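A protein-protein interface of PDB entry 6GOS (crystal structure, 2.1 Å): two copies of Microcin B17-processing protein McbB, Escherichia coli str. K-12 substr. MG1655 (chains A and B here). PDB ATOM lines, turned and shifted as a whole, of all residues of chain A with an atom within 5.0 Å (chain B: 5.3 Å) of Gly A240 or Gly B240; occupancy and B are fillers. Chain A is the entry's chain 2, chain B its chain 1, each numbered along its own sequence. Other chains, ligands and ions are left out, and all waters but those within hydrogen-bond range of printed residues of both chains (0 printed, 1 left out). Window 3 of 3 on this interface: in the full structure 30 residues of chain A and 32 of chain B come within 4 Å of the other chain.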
ATOM      1  N   GLU A 236     -23.214  27.256 -28.736  1.00  0.00           N
ATOM      2  CA  GLU A 236     -23.517  26.922 -27.336  1.00  0.00           C
ATOM      3  C   GLU A 236     -22.738  25.687 -26.822  1.00  0.00           C
ATOM      4  O   GLU A 236     -22.320  25.643 -25.653  1.00  0.00           O
ATOM      5  CB  GLU A 236     -25.028  26.696 -27.146  1.00  0.00           C
ATOM      6  CG  GLU A 236     -25.475  26.390 -25.699  1.00  0.00           C
ATOM      7  CD  GLU A 236     -26.944  25.977 -25.578  1.00  0.00           C
ATOM      8  OE1 GLU A 236     -27.789  26.381 -26.413  1.00  0.00           O
ATOM      9  OE2 GLU A 236     -27.253  25.231 -24.624  1.00  0.00           O
ATOM     10  N   SER A 237     -22.567  24.680 -27.664  1.00  0.00           N
ATOM     11  CA  SER A 237     -21.923  23.447 -27.218  1.00  0.00           C
ATOM     12  C   SER A 237     -20.437  23.656 -26.910  1.00  0.00           C
ATOM     13  O   SER A 237     -19.949  23.204 -25.873  1.00  0.00           O
ATOM     14  CB  SER A 237     -22.192  22.273 -28.174  1.00  0.00           C
ATOM     15  OG  SER A 237     -21.452  22.369 -29.356  1.00  0.00           O
ATOM     16  N   GLU A 238     -19.750  24.412 -27.771  1.00  0.00           N
ATOM     17  CA  GLU A 238     -18.358  24.740 -27.536  1.00  0.00           C
ATOM     18  C   GLU A 238     -18.202  25.553 -26.250  1.00  0.00           C
ATOM     19  O   GLU A 238     -17.279  25.320 -25.481  1.00  0.00           O
ATOM     20  CB  GLU A 238     -17.760  25.509 -28.699  1.00  0.00           C
ATOM     21  CG  GLU A 238     -17.554  24.681 -29.959  1.00  0.00           C
ATOM     22  CD  GLU A 238     -18.816  24.473 -30.778  1.00  0.00           C
ATOM     23  OE1 GLU A 238     -19.772  25.281 -30.669  1.00  0.00           O
ATOM     24  OE2 GLU A 238     -18.853  23.481 -31.529  1.00  0.00           O
ATOM     25  N   ARG A 239     -19.111  26.477 -26.002  1.00  0.00           N
ATOM     26  CA  ARG A 239     -19.053  27.247 -24.769  1.00  0.00           C
ATOM     27  C   ARG A 239     -19.362  26.413 -23.526  1.00  0.00           C
ATOM     28  O   ARG A 239     -18.728  26.612 -22.494  1.00  0.00           O
ATOM     29  CB  ARG A 239     -19.980  28.450 -24.829  1.00  0.00           C
ATOM     30  CG  ARG A 239     -19.500  29.498 -25.827  1.00  0.00           C
ATOM     31  CD  ARG A 239     -20.602  30.488 -26.145  1.00  0.00           C
ATOM     32  NE  ARG A 239     -20.043  31.585 -26.915  1.00  0.00           N
ATOM     33  CZ  ARG A 239     -20.502  32.041 -28.067  1.00  0.00           C
ATOM     34  NH1 ARG A 239     -21.618  31.577 -28.617  1.00  0.00           N
ATOM     35  NH2 ARG A 239     -19.851  33.041 -28.654  1.00  0.00           N
ATOM     36  N   GLY A 240     -20.326  25.501 -23.619  1.00  0.00           N
ATOM     37  CA  GLY A 240     -20.636  24.609 -22.499  1.00  0.00           C
ATOM     38  C   GLY A 240     -19.469  23.698 -22.201  1.00  0.00           C
ATOM     39  O   GLY A 240     -19.127  23.498 -21.059  1.00  0.00           O
ATOM     40  N   PHE A 241     -18.837  23.164 -23.238  1.00  0.00           N
ATOM     41  CA  PHE A 241     -17.601  22.408 -23.084  1.00  0.00           C
ATOM     42  C   PHE A 241     -16.491  23.225 -22.398  1.00  0.00           C
ATOM     43  O   PHE A 241     -15.812  22.745 -21.473  1.00  0.00           O
ATOM     44  CB  PHE A 241     -17.178  21.938 -24.474  1.00  0.00           C
ATOM     45  CG  PHE A 241     -15.945  21.091 -24.521  1.00  0.00           C
ATOM     46  CD1 PHE A 241     -16.003  19.735 -24.257  1.00  0.00           C
ATOM     47  CD2 PHE A 241     -14.761  21.622 -24.953  1.00  0.00           C
ATOM     48  CE1 PHE A 241     -14.881  18.948 -24.368  1.00  0.00           C
ATOM     49  CE2 PHE A 241     -13.646  20.831 -25.086  1.00  0.00           C
ATOM     50  CZ  PHE A 241     -13.699  19.506 -24.779  1.00  0.00           C
ATOM     51  N   SER A 242     -16.318  24.465 -22.837  1.00  0.00           N
ATOM     52  CA  SER A 242     -15.325  25.382 -22.235  1.00  0.00           C
ATOM     53  C   SER A 242     -15.633  25.657 -20.755  1.00  0.00           C
ATOM     54  O   SER A 242     -14.740  25.686 -19.920  1.00  0.00           O
ATOM     55  CB  SER A 242     -15.281  26.724 -23.000  1.00  0.00           C
ATOM     56  OG  SER A 242     -14.894  26.521 -24.362  1.00  0.00           O
ATOM     57  N   TYR A 243     -16.907  25.883 -20.472  1.00  0.00           N
ATOM     58  CA  TYR A 243     -17.404  26.190 -19.132  1.00  0.00           C
ATOM     59  C   TYR A 243     -17.007  25.093 -18.121  1.00  0.00           C
ATOM     60  O   TYR A 243     -16.491  25.375 -17.040  1.00  0.00           O
ATOM     61  CB  TYR A 243     -18.925  26.332 -19.245  1.00  0.00           C
ATOM     62  CG  TYR A 243     -19.710  26.769 -18.030  1.00  0.00           C
ATOM     63  CD1 TYR A 243     -19.717  28.101 -17.618  1.00  0.00           C
ATOM     64  CD2 TYR A 243     -20.505  25.872 -17.339  1.00  0.00           C
ATOM     65  CE1 TYR A 243     -20.489  28.523 -16.538  1.00  0.00           C
ATOM     66  CE2 TYR A 243     -21.287  26.281 -16.265  1.00  0.00           C
ATOM     67  CZ  TYR A 243     -21.272  27.602 -15.863  1.00  0.00           C
ATOM     68  OH  TYR A 243     -22.049  28.011 -14.794  1.00  0.00           O
ATOM     69  N   HIS A 244     -17.214  23.841 -18.515  1.00  0.00           N
ATOM     70  CA  HIS A 244     -16.889  22.694 -17.670  1.00  0.00           C
ATOM     71  C   HIS A 244     -15.383  22.521 -17.492  1.00  0.00           C
ATOM     72  O   HIS A 244     -14.941  22.260 -16.394  1.00  0.00           O
ATOM     73  CB  HIS A 244     -17.537  21.427 -18.241  1.00  0.00           C
ATOM     74  CG  HIS A 244     -17.293  20.200 -17.432  1.00  0.00           C
ATOM     75  ND1 HIS A 244     -17.915  19.966 -16.224  1.00  0.00           N
ATOM     76  CD2 HIS A 244     -16.502  19.128 -17.666  1.00  0.00           C
ATOM     77  CE1 HIS A 244     -17.517  18.797 -15.749  1.00  0.00           C
ATOM     78  NE2 HIS A 244     -16.671  18.262 -16.609  1.00  0.00           N
ATOM     79  N   GLY B 235     -24.529  18.773 -12.732  1.00  0.00           N
ATOM     80  CA  GLY B 235     -24.740  20.215 -12.717  1.00  0.00           C
ATOM     81  C   GLY B 235     -24.824  20.648 -14.171  1.00  0.00           C
ATOM     82  O   GLY B 235     -24.718  19.806 -15.091  1.00  0.00           O
ATOM     83  N   GLU B 236     -25.012  21.950 -14.378  1.00  0.00           N
ATOM     84  CA  GLU B 236     -25.100  22.540 -15.723  1.00  0.00           C
ATOM     85  C   GLU B 236     -23.837  22.306 -16.555  1.00  0.00           C
ATOM     86  O   GLU B 236     -23.929  22.038 -17.761  1.00  0.00           O
ATOM     87  CB  GLU B 236     -25.414  24.045 -15.631  1.00  0.00           C
ATOM     88  CG  GLU B 236     -25.864  24.672 -16.949  1.00  0.00           C
ATOM     89  CD  GLU B 236     -25.491  26.153 -17.108  1.00  0.00           C
ATOM     90  OE1 GLU B 236     -26.099  26.999 -16.418  1.00  0.00           O
ATOM     91  OE2 GLU B 236     -24.594  26.475 -17.938  1.00  0.00           O
ATOM     92  N   SER B 237     -22.658  22.394 -15.932  1.00  0.00           N
ATOM     93  CA  SER B 237     -21.387  22.213 -16.678  1.00  0.00           C
ATOM     94  C   SER B 237     -21.265  20.784 -17.189  1.00  0.00           C
ATOM     95  O   SER B 237     -20.932  20.567 -18.352  1.00  0.00           O
ATOM     96  CB  SER B 237     -20.159  22.599 -15.844  1.00  0.00           C
ATOM     97  OG  SER B 237     -19.884  21.632 -14.842  1.00  0.00           O
ATOM     98  N   GLU B 238     -21.566  19.800 -16.349  1.00  0.00           N
ATOM     99  CA  GLU B 238     -21.577  18.402 -16.818  1.00  0.00           C
ATOM    100  C   GLU B 238     -22.523  18.203 -18.009  1.00  0.00           C
ATOM    101  O   GLU B 238     -22.174  17.544 -18.985  1.00  0.00           O
ATOM    102  CB  GLU B 238     -21.942  17.422 -15.699  1.00  0.00           C
ATOM    103  CG  GLU B 238     -20.825  17.145 -14.690  1.00  0.00           C
ATOM    104  CD  GLU B 238     -20.644  18.228 -13.660  1.00  0.00           C
ATOM    105  OE1 GLU B 238     -21.602  18.972 -13.381  1.00  0.00           O
ATOM    106  OE2 GLU B 238     -19.527  18.346 -13.116  1.00  0.00           O
ATOM    107  N   ARG B 239     -23.707  18.791 -17.923  1.00  0.00           N
ATOM    108  CA  ARG B 239     -24.675  18.731 -19.029  1.00  0.00           C
ATOM    109  C   ARG B 239     -24.170  19.401 -20.298  1.00  0.00           C
ATOM    110  O   ARG B 239     -24.358  18.865 -21.391  1.00  0.00           O
ATOM    111  CB  ARG B 239     -26.007  19.374 -18.614  1.00  0.00           C
ATOM    112  CG  ARG B 239     -26.767  18.543 -17.615  1.00  0.00           C
ATOM    113  CD  ARG B 239     -28.035  19.214 -17.139  1.00  0.00           C
ATOM    114  NE  ARG B 239     -28.721  18.299 -16.231  1.00  0.00           N
ATOM    115  CZ  ARG B 239     -28.832  18.429 -14.904  1.00  0.00           C
ATOM    116  NH1 ARG B 239     -28.350  19.482 -14.244  1.00  0.00           N
ATOM    117  NH2 ARG B 239     -29.464  17.484 -14.218  1.00  0.00           N
ATOM    118  N   GLY B 240     -23.535  20.569 -20.153  1.00  0.00           N
ATOM    119  CA  GLY B 240     -22.976  21.294 -21.308  1.00  0.00           C
ATOM    120  C   GLY B 240     -21.865  20.526 -22.002  1.00  0.00           C
ATOM    121  O   GLY B 240     -21.803  20.468 -23.231  1.00  0.00           O
ATOM    122  N   PHE B 241     -20.999  19.931 -21.194  1.00  0.00           N
ATOM    123  CA  PHE B 241     -19.926  19.049 -21.663  1.00  0.00           C
ATOM    124  C   PHE B 241     -20.528  17.867 -22.435  1.00  0.00           C
ATOM    125  O   PHE B 241     -20.087  17.572 -23.552  1.00  0.00           O
ATOM    126  CB  PHE B 241     -19.087  18.585 -20.444  1.00  0.00           C
ATOM    127  CG  PHE B 241     -17.910  17.712 -20.785  1.00  0.00           C
ATOM    128  CD1 PHE B 241     -16.709  18.270 -21.243  1.00  0.00           C
ATOM    129  CD2 PHE B 241     -17.979  16.349 -20.632  1.00  0.00           C
ATOM    130  CE1 PHE B 241     -15.610  17.469 -21.536  1.00  0.00           C
ATOM    131  CE2 PHE B 241     -16.886  15.547 -20.944  1.00  0.00           C
ATOM    132  CZ  PHE B 241     -15.699  16.112 -21.405  1.00  0.00           C
ATOM    133  N   SER B 242     -21.554  17.237 -21.854  1.00  0.00           N
ATOM    134  CA  SER B 242     -22.261  16.111 -22.486  1.00  0.00           C
ATOM    135  C   SER B 242     -22.920  16.496 -23.820  1.00  0.00           C
ATOM    136  O   SER B 242     -22.862  15.760 -24.796  1.00  0.00           O
ATOM    137  CB  SER B 242     -23.331  15.539 -21.523  1.00  0.00           C
ATOM    138  OG  SER B 242     -22.768  15.091 -20.296  1.00  0.00           O
ATOM    139  N   TYR B 243     -23.525  17.675 -23.830  1.00  0.00           N
ATOM    140  CA  TYR B 243     -24.172  18.249 -24.996  1.00  0.00           C
ATOM    141  C   TYR B 243     -23.188  18.395 -26.170  1.00  0.00           C
ATOM    142  O   TYR B 243     -23.517  18.031 -27.300  1.00  0.00           O
ATOM    143  CB  TYR B 243     -24.738  19.608 -24.574  1.00  0.00           C
ATOM    144  CG  TYR B 243     -25.629  20.323 -25.539  1.00  0.00           C
ATOM    145  CD1 TYR B 243     -26.953  19.915 -25.737  1.00  0.00           C
ATOM    146  CD2 TYR B 243     -25.181  21.464 -26.212  1.00  0.00           C
ATOM    147  CE1 TYR B 243     -27.789  20.606 -26.595  1.00  0.00           C
ATOM    148  CE2 TYR B 243     -26.015  22.155 -27.078  1.00  0.00           C
ATOM    149  CZ  TYR B 243     -27.319  21.720 -27.253  1.00  0.00           C
ATOM    150  OH  TYR B 243     -28.134  22.410 -28.094  1.00  0.00           O
ATOM    151  N   HIS B 244     -21.978  18.896 -25.886  1.00  0.00           N
ATOM    152  CA  HIS B 244     -20.952  19.018 -26.918  1.00  0.00           C
ATOM    153  C   HIS B 244     -20.475  17.671 -27.459  1.00  0.00           C
ATOM    154  O   HIS B 244     -20.273  17.527 -28.673  1.00  0.00           O
ATOM    155  CB  HIS B 244     -19.762  19.865 -26.427  1.00  0.00           C
ATOM    156  CG  HIS B 244     -18.773  20.205 -27.508  1.00  0.00           C
ATOM    157  ND1 HIS B 244     -19.108  20.925 -28.639  1.00  0.00           N
ATOM    158  CD2 HIS B 244     -17.457  19.921 -27.622  1.00  0.00           C
ATOM    159  CE1 HIS B 244     -18.037  21.070 -29.398  1.00  0.00           C
ATOM    160  NE2 HIS B 244     -17.021  20.474 -28.800  1.00  0.00           N
ATOM    161  N   LEU B 245     -20.282  16.701 -26.573  1.00  0.00           N
ATOM    162  CA  LEU B 245     -19.844  15.363 -26.985  1.00  0.00           C
ATOM    163  C   LEU B 245     -20.887  14.673 -27.867  1.00  0.00           C
ATOM    164  O   LEU B 245     -20.541  14.063 -28.870  1.00  0.00           O
ATOM    165  CB  LEU B 245     -19.512  14.499 -25.771  1.00  0.00           C
ATOM    166  CG  LEU B 245     -18.284  14.880 -24.940  1.00  0.00           C
ATOM    167  CD1 LEU B 245     -18.079  13.898 -23.790  1.00  0.00           C
ATOM    168  CD2 LEU B 245     -17.054  14.912 -25.818  1.00  0.00           C
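OG of Ser B237 lies within hydrogen-bond range of ND1 of His A244 (2.9 Å).
A ring nitrogen (ND1) of His B244 sits at hydrogen-bond distance from the side-chain hydroxyl (OG) of Ser A237 (2.8 Å).
N of Gly B235 sits at hydrogen-bond distance from OE1 of Glu B238 (3.0 Å).
The side-chain hydroxyl (OG) of Ser B237 is in hydrogen-bond range of the side-chain carboxylate (OE1) of Glu B238, at 3.5 Å.
O of Glu B238 lies within hydrogen-bond range of OG of Ser B242 (2.8 Å).
The backbone carbonyl oxygen (O) of Glu A238 is in hydrogen-bond range of the side-chain hydroxyl (OG) of Ser A242, at 2.9 Å.
Among the printed residues, pairs that only touch across the chains: Phe A241 with Phe B241, Glu A238 with His B244, His A244 with Glu B238, Tyr A243 with Ser B237, Phe A241 with His B244, Ser A237 with Tyr B243, His A244 with Phe B241, Tyr A243 with Glu B236 and Gly A240 with Gly B240.
Glu A236 touches none of the printed residues of chain B.
Printed residues of chain B within 4 Å of Ser A237: Tyr B243 (3.7 Å) and His B244 (2.8 Å).
Of the printed residues of chain B, Glu A238 touches His B244 (3.3 Å).
Arg A239 touches none of the printed residues of chain B.
Of the printed residues of chain B, Gly A240 touches Gly B240 (3.98 Å).
Of the printed residues of chain B, Tyr A243 touches Glu B236 and Ser B237.
Of the printed residues of chain A, Ser B237 touches Tyr A243 and His A244.
Of the printed residues of chain A, Gly B240 touches Gly A240 (3.98 Å).
Of the printed residues of chain A, His B244 touches Ser A237 (2.8 Å), Glu A238 (3.3 Å) and Phe A241 (3.6 Å).
The nearest printed residue of chain B that does not touch Gly A240 is Phe B241 (4.03 Å).
Of the 11 printed residues of chain B, 7 touch a printed residue of chain A.
Along chain B the printed residues that touch a printed residue of chain A span positions 236 to 244.
Hydrophobic or aromatic side chains of chain A that line the printed part of chain B: Phe A241, Tyr A243 and His A244.
Among the printed residues, no Asp or Glu carboxylate lies within 4 Å of a Lys or Arg side-chain nitrogen of the other chain.
Ser A237 touches Tyr B243, and with the chains exchanged Tyr A243 touches Ser B237.
Ser A237 touches His B244, and with the chains exchanged His A244 touches Ser B237.
Glu A238 touches His B244, and with the chains exchanged His A244 touches Glu B238.
Gly A240 touches its own counterpart, Gly B240.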
